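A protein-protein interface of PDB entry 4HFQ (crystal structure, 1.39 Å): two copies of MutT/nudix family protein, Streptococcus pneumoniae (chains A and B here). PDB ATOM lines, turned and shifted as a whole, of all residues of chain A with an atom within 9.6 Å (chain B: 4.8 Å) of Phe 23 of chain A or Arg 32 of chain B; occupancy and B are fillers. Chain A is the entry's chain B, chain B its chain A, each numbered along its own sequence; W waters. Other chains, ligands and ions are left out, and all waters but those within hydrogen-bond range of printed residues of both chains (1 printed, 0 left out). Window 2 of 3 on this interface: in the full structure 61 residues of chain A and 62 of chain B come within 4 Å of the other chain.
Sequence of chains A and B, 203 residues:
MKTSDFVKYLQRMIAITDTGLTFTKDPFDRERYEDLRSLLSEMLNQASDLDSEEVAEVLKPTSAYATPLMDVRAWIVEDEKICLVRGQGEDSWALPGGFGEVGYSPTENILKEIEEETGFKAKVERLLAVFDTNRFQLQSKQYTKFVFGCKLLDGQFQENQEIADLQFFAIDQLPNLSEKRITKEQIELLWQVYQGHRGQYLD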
ATOM      1  N   ARG A  12      -6.983  -8.138  29.903  1.00  0.00           N
ATOM      2  CA  ARG A  12      -6.150  -8.585  28.793  1.00  0.00           C
ATOM      3  C   ARG A  12      -6.467  -7.796  27.520  1.00  0.00           C
ATOM      4  O   ARG A  12      -5.564  -7.415  26.773  1.00  0.00           O
ATOM      5  CB  ARG A  12      -6.310 -10.085  28.569  1.00  0.00           C
ATOM      6  CG  ARG A  12      -5.648 -10.906  29.680  1.00  0.00           C
ATOM      7  CD  ARG A  12      -5.877 -12.392  29.492  1.00  0.00           C
ATOM      8  NE  ARG A  12      -5.415 -13.127  30.676  1.00  0.00           N
ATOM      9  CZ  ARG A  12      -5.419 -14.452  30.781  1.00  0.00           C
ATOM     10  NH1 ARG A  12      -5.846 -15.206  29.781  1.00  0.00           N
ATOM     11  NH2 ARG A  12      -4.997 -15.013  31.902  1.00  0.00           N
ATOM     12  N   MET A  13      -7.750  -7.520  27.298  1.00  0.00           N
ATOM     13  CA  MET A  13      -8.141  -6.731  26.138  1.00  0.00           C
ATOM     14  C   MET A  13      -7.740  -5.270  26.272  1.00  0.00           C
ATOM     15  O   MET A  13      -7.322  -4.646  25.287  1.00  0.00           O
ATOM     16  CB  MET A  13      -9.637  -6.850  25.890  1.00  0.00           C
ATOM     17  CG  MET A  13     -10.036  -8.254  25.419  1.00  0.00           C
ATOM     18  SD  MET A  13     -11.747  -8.390  24.870  1.00  0.00           S
ATOM     19  CE  MET A  13     -12.546  -8.340  26.423  1.00  0.00           C
ATOM     20  N   ILE A  14      -7.843  -4.715  27.483  1.00  0.00           N
ATOM     21  CA  ILE A  14      -7.383  -3.365  27.734  1.00  0.00           C
ATOM     22  C   ILE A  14      -5.887  -3.243  27.465  1.00  0.00           C
ATOM     23  O   ILE A  14      -5.443  -2.246  26.885  1.00  0.00           O
ATOM     24  CB  ILE A  14      -7.759  -2.923  29.166  1.00  0.00           C
ATOM     25  CG1 ILE A  14      -9.279  -2.673  29.237  1.00  0.00           C
ATOM     26  CG2 ILE A  14      -6.981  -1.670  29.565  1.00  0.00           C
ATOM     27  CD1 ILE A  14      -9.844  -2.601  30.654  1.00  0.00           C
ATOM     28  N   ALA A  15      -5.095  -4.230  27.884  1.00  0.00           N
ATOM     29  CA  ALA A  15      -3.646  -4.197  27.604  1.00  0.00           C
ATOM     30  C   ALA A  15      -3.354  -4.032  26.121  1.00  0.00           C
ATOM     31  O   ALA A  15      -2.534  -3.206  25.721  1.00  0.00           O
ATOM     32  CB  ALA A  15      -2.951  -5.441  28.144  1.00  0.00           C
ATOM     33  N   ILE A  16      -4.025  -4.827  25.294  1.00  0.00           N
ATOM     34  CA  ILE A  16      -3.793  -4.761  23.865  1.00  0.00           C
ATOM     35  C   ILE A  16      -4.259  -3.415  23.305  1.00  0.00           C
ATOM     36  O   ILE A  16      -3.573  -2.790  22.489  1.00  0.00           O
ATOM     37  CB  ILE A  16      -4.528  -5.902  23.135  1.00  0.00           C
ATOM     38  CG1 ILE A  16      -3.931  -7.264  23.492  1.00  0.00           C
ATOM     39  CG2 ILE A  16      -4.468  -5.669  21.622  1.00  0.00           C
ATOM     40  CD1 ILE A  16      -4.911  -8.400  23.327  1.00  0.00           C
ATOM     41  N   THR A  17      -5.424  -2.958  23.748  1.00  0.00           N
ATOM     42  CA  THR A  17      -5.971  -1.699  23.285  1.00  0.00           C
ATOM     43  C   THR A  17      -5.051  -0.534  23.641  1.00  0.00           C
ATOM     44  O   THR A  17      -4.807   0.356  22.797  1.00  0.00           O
ATOM     45  CB  THR A  17      -7.399  -1.503  23.824  1.00  0.00           C
ATOM     46  OG1 THR A  17      -8.217  -2.627  23.421  1.00  0.00           O
ATOM     47  CG2 THR A  17      -7.997  -0.251  23.302  1.00  0.00           C
ATOM     48  N   ASP A  18      -4.515  -0.553  24.866  1.00  0.00           N
ATOM     49  CA  ASP A  18      -3.577   0.480  25.291  1.00  0.00           C
ATOM     50  C   ASP A  18      -2.308   0.480  24.445  1.00  0.00           C
ATOM     51  O   ASP A  18      -1.780   1.550  24.130  1.00  0.00           O
ATOM     52  CB  ASP A  18      -3.227   0.293  26.764  1.00  0.00           C
ATOM     53  CG  ASP A  18      -4.316   0.758  27.691  1.00  0.00           C
ATOM     54  OD1 ASP A  18      -5.269   1.423  27.259  1.00  0.00           O
ATOM     55  OD2 ASP A  18      -4.208   0.465  28.907  1.00  0.00           O
ATOM     56  N   THR A  19      -1.837  -0.698  24.089  1.00  0.00           N
ATOM     57  CA  THR A  19      -0.707  -0.817  23.205  1.00  0.00           C
ATOM     58  C   THR A  19      -1.037  -0.112  21.881  1.00  0.00           C
ATOM     59  O   THR A  19      -0.240   0.703  21.398  1.00  0.00           O
ATOM     60  CB  THR A  19      -0.315  -2.300  23.072  1.00  0.00           C
ATOM     61  OG1 THR A  19       0.026  -2.803  24.382  1.00  0.00           O
ATOM     62  CG2 THR A  19       0.854  -2.478  22.159  1.00  0.00           C
ATOM     63  N   GLY A  20      -2.224  -0.378  21.320  1.00  0.00           N
ATOM     64  CA  GLY A  20      -2.664   0.258  20.083  1.00  0.00           C
ATOM     65  C   GLY A  20      -2.673   1.768  20.219  1.00  0.00           C
ATOM     66  O   GLY A  20      -2.177   2.480  19.339  1.00  0.00           O
ATOM     67  N   LEU A  21      -3.224   2.274  21.327  1.00  0.00           N
ATOM     68  CA  LEU A  21      -3.278   3.710  21.553  1.00  0.00           C
ATOM     69  C   LEU A  21      -1.883   4.341  21.616  1.00  0.00           C
ATOM     70  O   LEU A  21      -1.716   5.490  21.196  1.00  0.00           O
ATOM     71  CB  LEU A  21      -4.047   4.024  22.847  1.00  0.00           C
ATOM     72  CG  LEU A  21      -5.556   3.786  22.733  1.00  0.00           C
ATOM     73  CD1 LEU A  21      -6.193   3.836  24.115  1.00  0.00           C
ATOM     74  CD2 LEU A  21      -6.247   4.776  21.790  1.00  0.00           C
ATOM     75  N   THR A  22      -0.899   3.635  22.158  1.00  0.00           N
ATOM     76  CA  THR A  22       0.467   4.184  22.196  1.00  0.00           C
ATOM     77  C   THR A  22       1.103   4.121  20.808  1.00  0.00           C
ATOM     78  O   THR A  22       1.673   5.120  20.341  1.00  0.00           O
ATOM     79  CB  THR A  22       1.359   3.455  23.220  1.00  0.00           C
ATOM     80  OG1 THR A  22       0.912   3.775  24.545  1.00  0.00           O
ATOM     81  CG2 THR A  22       2.822   3.896  23.098  1.00  0.00           C
ATOM     82  N   PHE A  23       1.012   2.970  20.149  1.00  0.00           N
ATOM     83  CA  PHE A  23       1.904   2.694  19.017  1.00  0.00           C
ATOM     84  C   PHE A  23       1.342   2.909  17.630  1.00  0.00           C
ATOM     85  O   PHE A  23       2.118   3.067  16.703  1.00  0.00           O
ATOM     86  CB  PHE A  23       2.503   1.297  19.149  1.00  0.00           C
ATOM     87  CG  PHE A  23       3.438   1.147  20.332  1.00  0.00           C
ATOM     88  CD1 PHE A  23       4.788   1.510  20.228  1.00  0.00           C
ATOM     89  CD2 PHE A  23       2.984   0.624  21.534  1.00  0.00           C
ATOM     90  CE1 PHE A  23       5.648   1.368  21.316  1.00  0.00           C
ATOM     91  CE2 PHE A  23       3.849   0.481  22.630  1.00  0.00           C
ATOM     92  CZ  PHE A  23       5.181   0.868  22.519  1.00  0.00           C
ATOM     93  N   THR A  24       0.025   2.886  17.454  1.00  0.00           N
ATOM     94  CA  THR A  24      -0.476   3.018  16.089  1.00  0.00           C
ATOM     95  C   THR A  24      -0.123   4.379  15.469  1.00  0.00           C
ATOM     96  O   THR A  24      -0.108   5.399  16.161  1.00  0.00           O
ATOM     97  CB  THR A  24      -1.993   2.753  15.961  1.00  0.00           C
ATOM     98  OG1 THR A  24      -2.287   2.568  14.573  1.00  0.00           O
ATOM     99  CG2 THR A  24      -2.851   3.902  16.502  1.00  0.00           C
ATOM    100  N   LYS A  25       0.086   4.362  14.157  1.00  0.00           N
ATOM    101  CA  LYS A  25       0.420   5.573  13.403  1.00  0.00           C
ATOM    102  C   LYS A  25      -0.731   6.004  12.507  1.00  0.00           C
ATOM    103  O   LYS A  25      -0.631   7.016  11.824  1.00  0.00           O
ATOM    104  CB  LYS A  25       1.703   5.367  12.579  1.00  0.00           C
ATOM    105  CG  LYS A  25       2.905   5.055  13.471  1.00  0.00           C
ATOM    106  CD  LYS A  25       4.164   4.758  12.655  1.00  0.00           C
ATOM    107  CE  LYS A  25       5.349   4.571  13.589  1.00  0.00           C
ATOM    108  NZ  LYS A  25       6.577   4.322  12.787  1.00  0.00           N
ATOM    109  N   ASP A  26      -1.833   5.258  12.542  1.00  0.00           N
ATOM    110  CA  ASP A  26      -2.962   5.469  11.627  1.00  0.00           C
ATOM    111  C   ASP A  26      -4.115   6.067  12.428  1.00  0.00           C
ATOM    112  O   ASP A  26      -4.525   5.493  13.431  1.00  0.00           O
ATOM    113  CB  ASP A  26      -3.313   4.093  11.006  1.00  0.00           C
ATOM    114  CG  ASP A  26      -4.538   4.099  10.083  1.00  0.00           C
ATOM    115  OD1 ASP A  26      -5.493   4.835  10.313  1.00  0.00           O
ATOM    116  OD2 ASP A  26      -4.569   3.250   9.156  1.00  0.00           O
ATOM    117  N   PRO A  27      -4.644   7.230  12.019  1.00  0.00           N
ATOM    118  CA  PRO A  27      -5.723   7.857  12.787  1.00  0.00           C
ATOM    119  C   PRO A  27      -7.025   7.032  12.875  1.00  0.00           C
ATOM    120  O   PRO A  27      -7.789   7.177  13.824  1.00  0.00           O
ATOM    121  CB  PRO A  27      -5.994   9.174  12.016  1.00  0.00           C
ATOM    122  CG  PRO A  27      -5.502   8.908  10.642  1.00  0.00           C
ATOM    123  CD  PRO A  27      -4.296   8.031  10.822  1.00  0.00           C
ATOM    124  N   ASP A  29      -7.135   3.625  12.889  1.00  0.00           N
ATOM    125  CA  ASP A  29      -6.833   2.636  13.938  1.00  0.00           C
ATOM    126  C   ASP A  29      -6.946   3.297  15.314  1.00  0.00           C
ATOM    127  O   ASP A  29      -7.558   2.727  16.224  1.00  0.00           O
ATOM    128  CB  ASP A  29      -5.449   2.017  13.737  1.00  0.00           C
ATOM    129  CG  ASP A  29      -5.420   1.006  12.641  1.00  0.00           C
ATOM    130  OD1 ASP A  29      -6.282   0.101  12.602  1.00  0.00           O
ATOM    131  OD2 ASP A  29      -4.484   1.093  11.826  1.00  0.00           O
ATOM    132  N   ARG A  30      -6.428   4.523  15.468  1.00  0.00           N
ATOM    133  CA  ARG A  30      -6.501   5.190  16.760  1.00  0.00           C
ATOM    134  C   ARG A  30      -7.958   5.346  17.190  1.00  0.00           C
ATOM    135  O   ARG A  30      -8.288   5.091  18.350  1.00  0.00           O
ATOM    136  CB  ARG A  30      -5.774   6.541  16.711  1.00  0.00           C
ATOM    137  CG  ARG A  30      -5.914   7.354  17.998  1.00  0.00           C
ATOM    138  CD  ARG A  30      -4.894   8.495  18.096  1.00  0.00           C
ATOM    139  NE  ARG A  30      -3.543   7.950  17.941  1.00  0.00           N
ATOM    140  CZ  ARG A  30      -2.877   7.304  18.902  1.00  0.00           C
ATOM    141  NH1 ARG A  30      -3.417   7.192  20.119  1.00  0.00           N
ATOM    142  NH2 ARG A  30      -1.661   6.790  18.640  1.00  0.00           N
ATOM    143  N   TYR A  33      -9.253   2.040  18.485  1.00  0.00           N
ATOM    144  CA  TYR A  33      -8.745   1.730  19.817  1.00  0.00           C
ATOM    145  C   TYR A  33      -9.369   2.628  20.872  1.00  0.00           C
ATOM    146  O   TYR A  33      -9.611   2.163  21.985  1.00  0.00           O
ATOM    147  CB  TYR A  33      -7.210   1.816  19.881  1.00  0.00           C
ATOM    148  CG  TYR A  33      -6.451   0.805  19.031  1.00  0.00           C
ATOM    149  CD1 TYR A  33      -6.683  -0.558  19.161  1.00  0.00           C
ATOM    150  CD2 TYR A  33      -5.498   1.241  18.136  1.00  0.00           C
ATOM    151  CE1 TYR A  33      -5.967  -1.475  18.417  1.00  0.00           C
ATOM    152  CE2 TYR A  33      -4.787   0.343  17.360  1.00  0.00           C
ATOM    153  CZ  TYR A  33      -5.022  -1.015  17.507  1.00  0.00           C
ATOM    154  OH  TYR A  33      -4.303  -1.924  16.766  1.00  0.00           O
ATOM    155  N   LEU A  36     -12.831   1.066  21.417  1.00  0.00           N
ATOM    156  CA  LEU A  36     -12.637  -0.151  22.217  1.00  0.00           C
ATOM    157  C   LEU A  36     -12.282   0.161  23.661  1.00  0.00           C
ATOM    158  O   LEU A  36     -12.838  -0.448  24.574  1.00  0.00           O
ATOM    159  CB  LEU A  36     -11.555  -1.034  21.610  1.00  0.00           C
ATOM    160  CG  LEU A  36     -11.944  -1.771  20.325  1.00  0.00           C
ATOM    161  CD1 LEU A  36     -10.685  -2.234  19.602  1.00  0.00           C
ATOM    162  CD2 LEU A  36     -12.874  -2.941  20.600  1.00  0.00           C
ATOM    163  N   PHE B  28       1.570  -4.828  12.995  1.00  0.00           N
ATOM    164  CA  PHE B  28       1.423  -4.896  14.442  1.00  0.00           C
ATOM    165  C   PHE B  28       0.003  -4.548  14.864  1.00  0.00           C
ATOM    166  O   PHE B  28      -0.506  -5.158  15.790  1.00  0.00           O
ATOM    167  CB  PHE B  28       2.449  -4.022  15.170  1.00  0.00           C
ATOM    168  CG  PHE B  28       3.875  -4.449  14.939  1.00  0.00           C
ATOM    169  CD1 PHE B  28       4.600  -3.915  13.877  1.00  0.00           C
ATOM    170  CD2 PHE B  28       4.490  -5.370  15.777  1.00  0.00           C
ATOM    171  CE1 PHE B  28       5.917  -4.296  13.654  1.00  0.00           C
ATOM    172  CE2 PHE B  28       5.818  -5.754  15.561  1.00  0.00           C
ATOM    173  CZ  PHE B  28       6.523  -5.218  14.496  1.00  0.00           C
ATOM    174  N   ASP B  29      -0.639  -3.622  14.160  1.00  0.00           N
ATOM    175  CA  ASP B  29      -2.071  -3.366  14.405  1.00  0.00           C
ATOM    176  C   ASP B  29      -2.906  -4.595  14.034  1.00  0.00           C
ATOM    177  O   ASP B  29      -3.785  -4.990  14.782  1.00  0.00           O
ATOM    178  CB  ASP B  29      -2.552  -2.138  13.638  1.00  0.00           C
ATOM    179  CG  ASP B  29      -2.121  -0.839  14.295  1.00  0.00           C
ATOM    180  OD1 ASP B  29      -2.331  -0.692  15.522  1.00  0.00           O
ATOM    181  OD2 ASP B  29      -1.598   0.041  13.582  1.00  0.00           O
ATOM    182  N   ARG B  30      -2.578  -5.239  12.909  1.00  0.00           N
ATOM    183  CA  ARG B  30      -3.283  -6.477  12.530  1.00  0.00           C
ATOM    184  C   ARG B  30      -3.204  -7.491  13.678  1.00  0.00           C
ATOM    185  O   ARG B  30      -4.212  -8.072  14.065  1.00  0.00           O
ATOM    186  CB  ARG B  30      -2.698  -7.074  11.250  1.00  0.00           C
ATOM    187  CG  ARG B  30      -3.299  -8.423  10.902  1.00  0.00           C
ATOM    188  CD  ARG B  30      -2.894  -8.856   9.497  1.00  0.00           C
ATOM    189  NE  ARG B  30      -3.461 -10.170   9.210  1.00  0.00           N
ATOM    190  CZ  ARG B  30      -4.715 -10.378   8.788  1.00  0.00           C
ATOM    191  NH1 ARG B  30      -5.529  -9.368   8.539  1.00  0.00           N
ATOM    192  NH2 ARG B  30      -5.133 -11.620   8.583  1.00  0.00           N
ATOM    193  N   GLU B  31      -2.005  -7.690  14.221  1.00  0.00           N
ATOM    194  CA  GLU B  31      -1.818  -8.639  15.303  1.00  0.00           C
ATOM    195  C   GLU B  31      -2.629  -8.262  16.532  1.00  0.00           C
ATOM    196  O   GLU B  31      -3.192  -9.123  17.181  1.00  0.00           O
ATOM    197  CB  GLU B  31      -0.352  -8.712  15.679  1.00  0.00           C
ATOM    198  CG  GLU B  31      -0.071  -9.768  16.723  1.00  0.00           C
ATOM    199  CD  GLU B  31       1.407  -9.885  17.021  1.00  0.00           C
ATOM    200  OE1 GLU B  31       2.109  -8.848  16.980  1.00  0.00           O
ATOM    201  OE2 GLU B  31       1.863 -11.018  17.286  1.00  0.00           O
ATOM    202  N   ARG B  32      -2.687  -6.969  16.840  1.00  0.00           N
ATOM    203  CA  ARG B  32      -3.507  -6.486  17.967  1.00  0.00           C
ATOM    204  C   ARG B  32      -4.979  -6.858  17.781  1.00  0.00           C
ATOM    205  O   ARG B  32      -5.601  -7.385  18.712  1.00  0.00           O
ATOM    206  CB  ARG B  32      -3.377  -4.981  18.161  1.00  0.00           C
ATOM    207  CG  ARG B  32      -2.043  -4.537  18.707  1.00  0.00           C
ATOM    208  CD  ARG B  32      -1.924  -3.008  18.698  1.00  0.00           C
ATOM    209  NE  ARG B  32      -0.539  -2.781  18.969  1.00  0.00           N
ATOM    210  CZ  ARG B  32       0.319  -2.140  18.199  1.00  0.00           C
ATOM    211  NH1 ARG B  32      -0.069  -1.430  17.130  1.00  0.00           N
ATOM    212  NH2 ARG B  32       1.561  -2.111  18.611  1.00  0.00           N
ATOM    213  N   TYR B  33      -5.532  -6.605  16.588  1.00  0.00           N
ATOM    214  CA  TYR B  33      -6.916  -6.977  16.342  1.00  0.00           C
ATOM    215  C   TYR B  33      -7.107  -8.491  16.401  1.00  0.00           C
ATOM    216  O   TYR B  33      -8.117  -8.954  16.912  1.00  0.00           O
ATOM    217  CB  TYR B  33      -7.431  -6.409  15.022  1.00  0.00           C
ATOM    218  CG  TYR B  33      -7.472  -4.899  14.941  1.00  0.00           C
ATOM    219  CD1 TYR B  33      -8.276  -4.149  15.818  1.00  0.00           C
ATOM    220  CD2 TYR B  33      -6.763  -4.225  13.959  1.00  0.00           C
ATOM    221  CE1 TYR B  33      -8.327  -2.758  15.731  1.00  0.00           C
ATOM    222  CE2 TYR B  33      -6.794  -2.840  13.874  1.00  0.00           C
ATOM    223  CZ  TYR B  33      -7.597  -2.119  14.739  1.00  0.00           C
ATOM    224  OH  TYR B  33      -7.660  -0.740  14.627  1.00  0.00           O
ATOM    225  N   GLU B  34      -6.139  -9.252  15.890  1.00  0.00           N
ATOM    226  CA  GLU B  34      -6.253 -10.710  15.939  1.00  0.00           C
ATOM    227  C   GLU B  34      -6.262 -11.202  17.388  1.00  0.00           C
ATOM    228  O   GLU B  34      -7.030 -12.090  17.753  1.00  0.00           O
ATOM    229  CB  GLU B  34      -5.130 -11.388  15.159  1.00  0.00           C
ATOM    230  CG  GLU B  34      -5.250 -11.202  13.661  1.00  0.00           C
ATOM    231  CD  GLU B  34      -4.103 -11.788  12.885  1.00  0.00           C
ATOM    232  OE1 GLU B  34      -2.956 -11.702  13.347  1.00  0.00           O
ATOM    233  OE2 GLU B  34      -4.356 -12.279  11.781  1.00  0.00           O
ATOM    234  N   ASP B  35      -5.390 -10.611  18.209  1.00  0.00           N
ATOM    235  CA  ASP B  35      -5.326 -10.970  19.623  1.00  0.00           C
ATOM    236  C   ASP B  35      -6.610 -10.579  20.361  1.00  0.00           C
ATOM    237  O   ASP B  35      -7.095 -11.317  21.209  1.00  0.00           O
ATOM    238  CB  ASP B  35      -4.097 -10.336  20.267  1.00  0.00           C
ATOM    239  CG  ASP B  35      -2.807 -10.964  19.788  1.00  0.00           C
ATOM    240  OD1 ASP B  35      -2.857 -12.064  19.193  1.00  0.00           O
ATOM    241  OD2 ASP B  35      -1.752 -10.329  20.027  1.00  0.00           O
ATOM    242  N   LEU B  36      -7.185  -9.425  20.005  1.00  0.00           N
ATOM    243  CA  LEU B  36      -8.468  -9.035  20.551  1.00  0.00           C
ATOM    244  C   LEU B  36      -9.557 -10.031  20.160  1.00  0.00           C
ATOM    245  O   LEU B  36     -10.369 -10.439  21.003  1.00  0.00           O
ATOM    246  CB  LEU B  36      -8.834  -7.610  20.102  1.00  0.00           C
ATOM    247  CG  LEU B  36      -8.040  -6.527  20.820  1.00  0.00           C
ATOM    248  CD1 LEU B  36      -8.227  -5.226  20.070  1.00  0.00           C
ATOM    249  CD2 LEU B  36      -8.443  -6.379  22.283  1.00  0.00           C
HETATM  250  O   HOH W   1       0.338   1.940  12.583  1.00  0.00           O
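Leu 36 of chain B touches Met 13 of chain A (CD2 to O, 3.6 Å).
CG2 of Ile 16 of chain A touches O of Arg 32 of chain B, 3.6 Å away.
Ile 16 of chain A touches Asp 35 of chain B (CD1 to CB, 3.7 Å).
Leu 36 of chain B touches Ile 16 of chain A (CG to CG2, 3.8 Å).
CD2 of Leu 36 of chain B touches OG1 of Thr 17 of chain A (3.9 Å).
Thr 19 of chain A touches Arg 32 of chain B.
Gly 20 of chain A touches Arg 32 of chain B (CA to CD, 3.6 Å).
Phe 23 of chain A touches Arg 32 of chain B (CB to NH2, 3.6 Å).
Tyr 33 of chain A touches Arg 32 of chain B.
Leu 36 of chain A touches Leu 36 of chain B (CD1 to CD1, 3.9 Å).
The side-chain carboxylate (OD2) of Asp 29 of chain B sits at hydrogen-bond distance from the side-chain hydroxyl (OG1) of Thr 24 of chain A.
The side-chain carboxylate of Asp 29 of chain A is in hydrogen-bond range of the side-chain hydroxyl of Tyr 33 of chain B.
OD1 of Asp 29 of chain B lies within hydrogen-bond range of OH of Tyr 33 of chain A (2.6 Å).
Water W1 lies within hydrogen-bond range of the side-chain carboxylate of Asp 29 of chain B (2.9 Å), the backbone NH of Lys 25 of chain A (2.9 Å) and the side-chain hydroxyl of Thr 24 of chain A (3.4 Å).
Asp 29 of chain A touches its own counterpart, Asp 29 of chain B.
Asp 29 of chain A touches Tyr 33 of chain B, and with the chains exchanged Tyr 33 of chain A touches Asp 29 of chain B.
Tyr 33 of chain B touches its own counterpart, Tyr 33 of chain A.
Leu 36 of chain A touches its own counterpart, Leu 36 of chain B.
Positions printed for both chains: 29, 30, 33 and 36.
Of the 15 pairs that touch across the chains among the printed residues, 5 have their exchanged pair printed and touching as well.
Phe 23 of chain A touches one residue of chain B.
Of the printed residues of chain A, Arg 32 of chain B touches Ile 16, Thr 19, Gly 20, Phe 23 and Tyr 33.
Of the printed residues of chain A, Asp 29 of chain B touches Thr 24, Asp 29 and Tyr 33.
Asp 35 of chain B touches just one residue of chain A: Ile 16.
Printed residues of chain B within 4 Å of Ile 16 of chain A: Arg 32, Asp 35 and Leu 36.
Of the printed residues of chain A, Leu 36 of chain B touches Met 13 (3.6 Å), Ile 16 (3.8 Å), Thr 17 (3.9 Å) and Leu 36 (3.9 Å).
Of the printed residues of chain B, Leu 36 of chain A touches Leu 36.
Of the printed residues of chain B, Tyr 33 of chain A touches Asp 29 (2.6 Å), Arg 32 (3.3 Å) and Tyr 33 (3.8 Å).
Ile 14 of chain A touches none of the printed residues of chain B.
Arg 12 of chain A touches none of the printed residues of chain B.
The nearest printed residue of chain B that does not touch Phe 23 of chain A is Asp 29 of chain B (5.6 Å).
The nearest printed residue of chain A that does not touch Arg 32 of chain B is Thr 24 of chain A (4.3 Å).
The nearest printed residue of chain B that does not touch Gly 20 of chain A is Asp 29 of chain B (4.7 Å).
The side-chain hydroxyl (OG1) of Thr 19 of chain A sits at hydrogen-bond distance from the backbone carbonyl oxygen (O) of Ala 15 of chain A (2.9 Å).
O of Met 13 of chain A is in hydrogen-bond range of OG1 of Thr 17 of chain A (2.9 Å).
The side-chain carboxylate (OD1) of Asp 26 of chain A lies within hydrogen-bond range of the backbone NH (N) of Asp 29 of chain A (3.3 Å).
O of Thr 24 of chain A is in hydrogen-bond range of NH2 of Arg 30 of chain A (3.2 Å).
NH1 of Arg 32 of chain B lies within salt-bridge range of OD1 of Asp 29 of chain B (2.9 Å).
The side-chain hydroxyl of Thr 24 of chain A is in hydrogen-bond range of the backbone NH of Asp 26 of chain A.
Of the 20 printed residues of chain A, 10 touch a printed residue of chain B.
Hydrophobic or aromatic side chains of chain A that line the printed part of chain B: Met 13, Ile 16, Phe 23, Tyr 33 and Leu 36.
Printed residues of chain B that touch a printed residue of chain A: Asp 29, Arg 32, Tyr 33, Asp 35 and Leu 36.
Hydrophobic or aromatic side chains of chain B within 4 Å of the printed part of chain A: Tyr 33 and Leu 36.
Along chain B the printed residues that touch a printed residue of chain A span positions 29 to 36.
Among the printed residues, 15 pairs touch across the chains.
Among the printed residues, no Asp or Glu carboxylate lies within 4 Å of a Lys or Arg side-chain nitrogen of the other chain.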
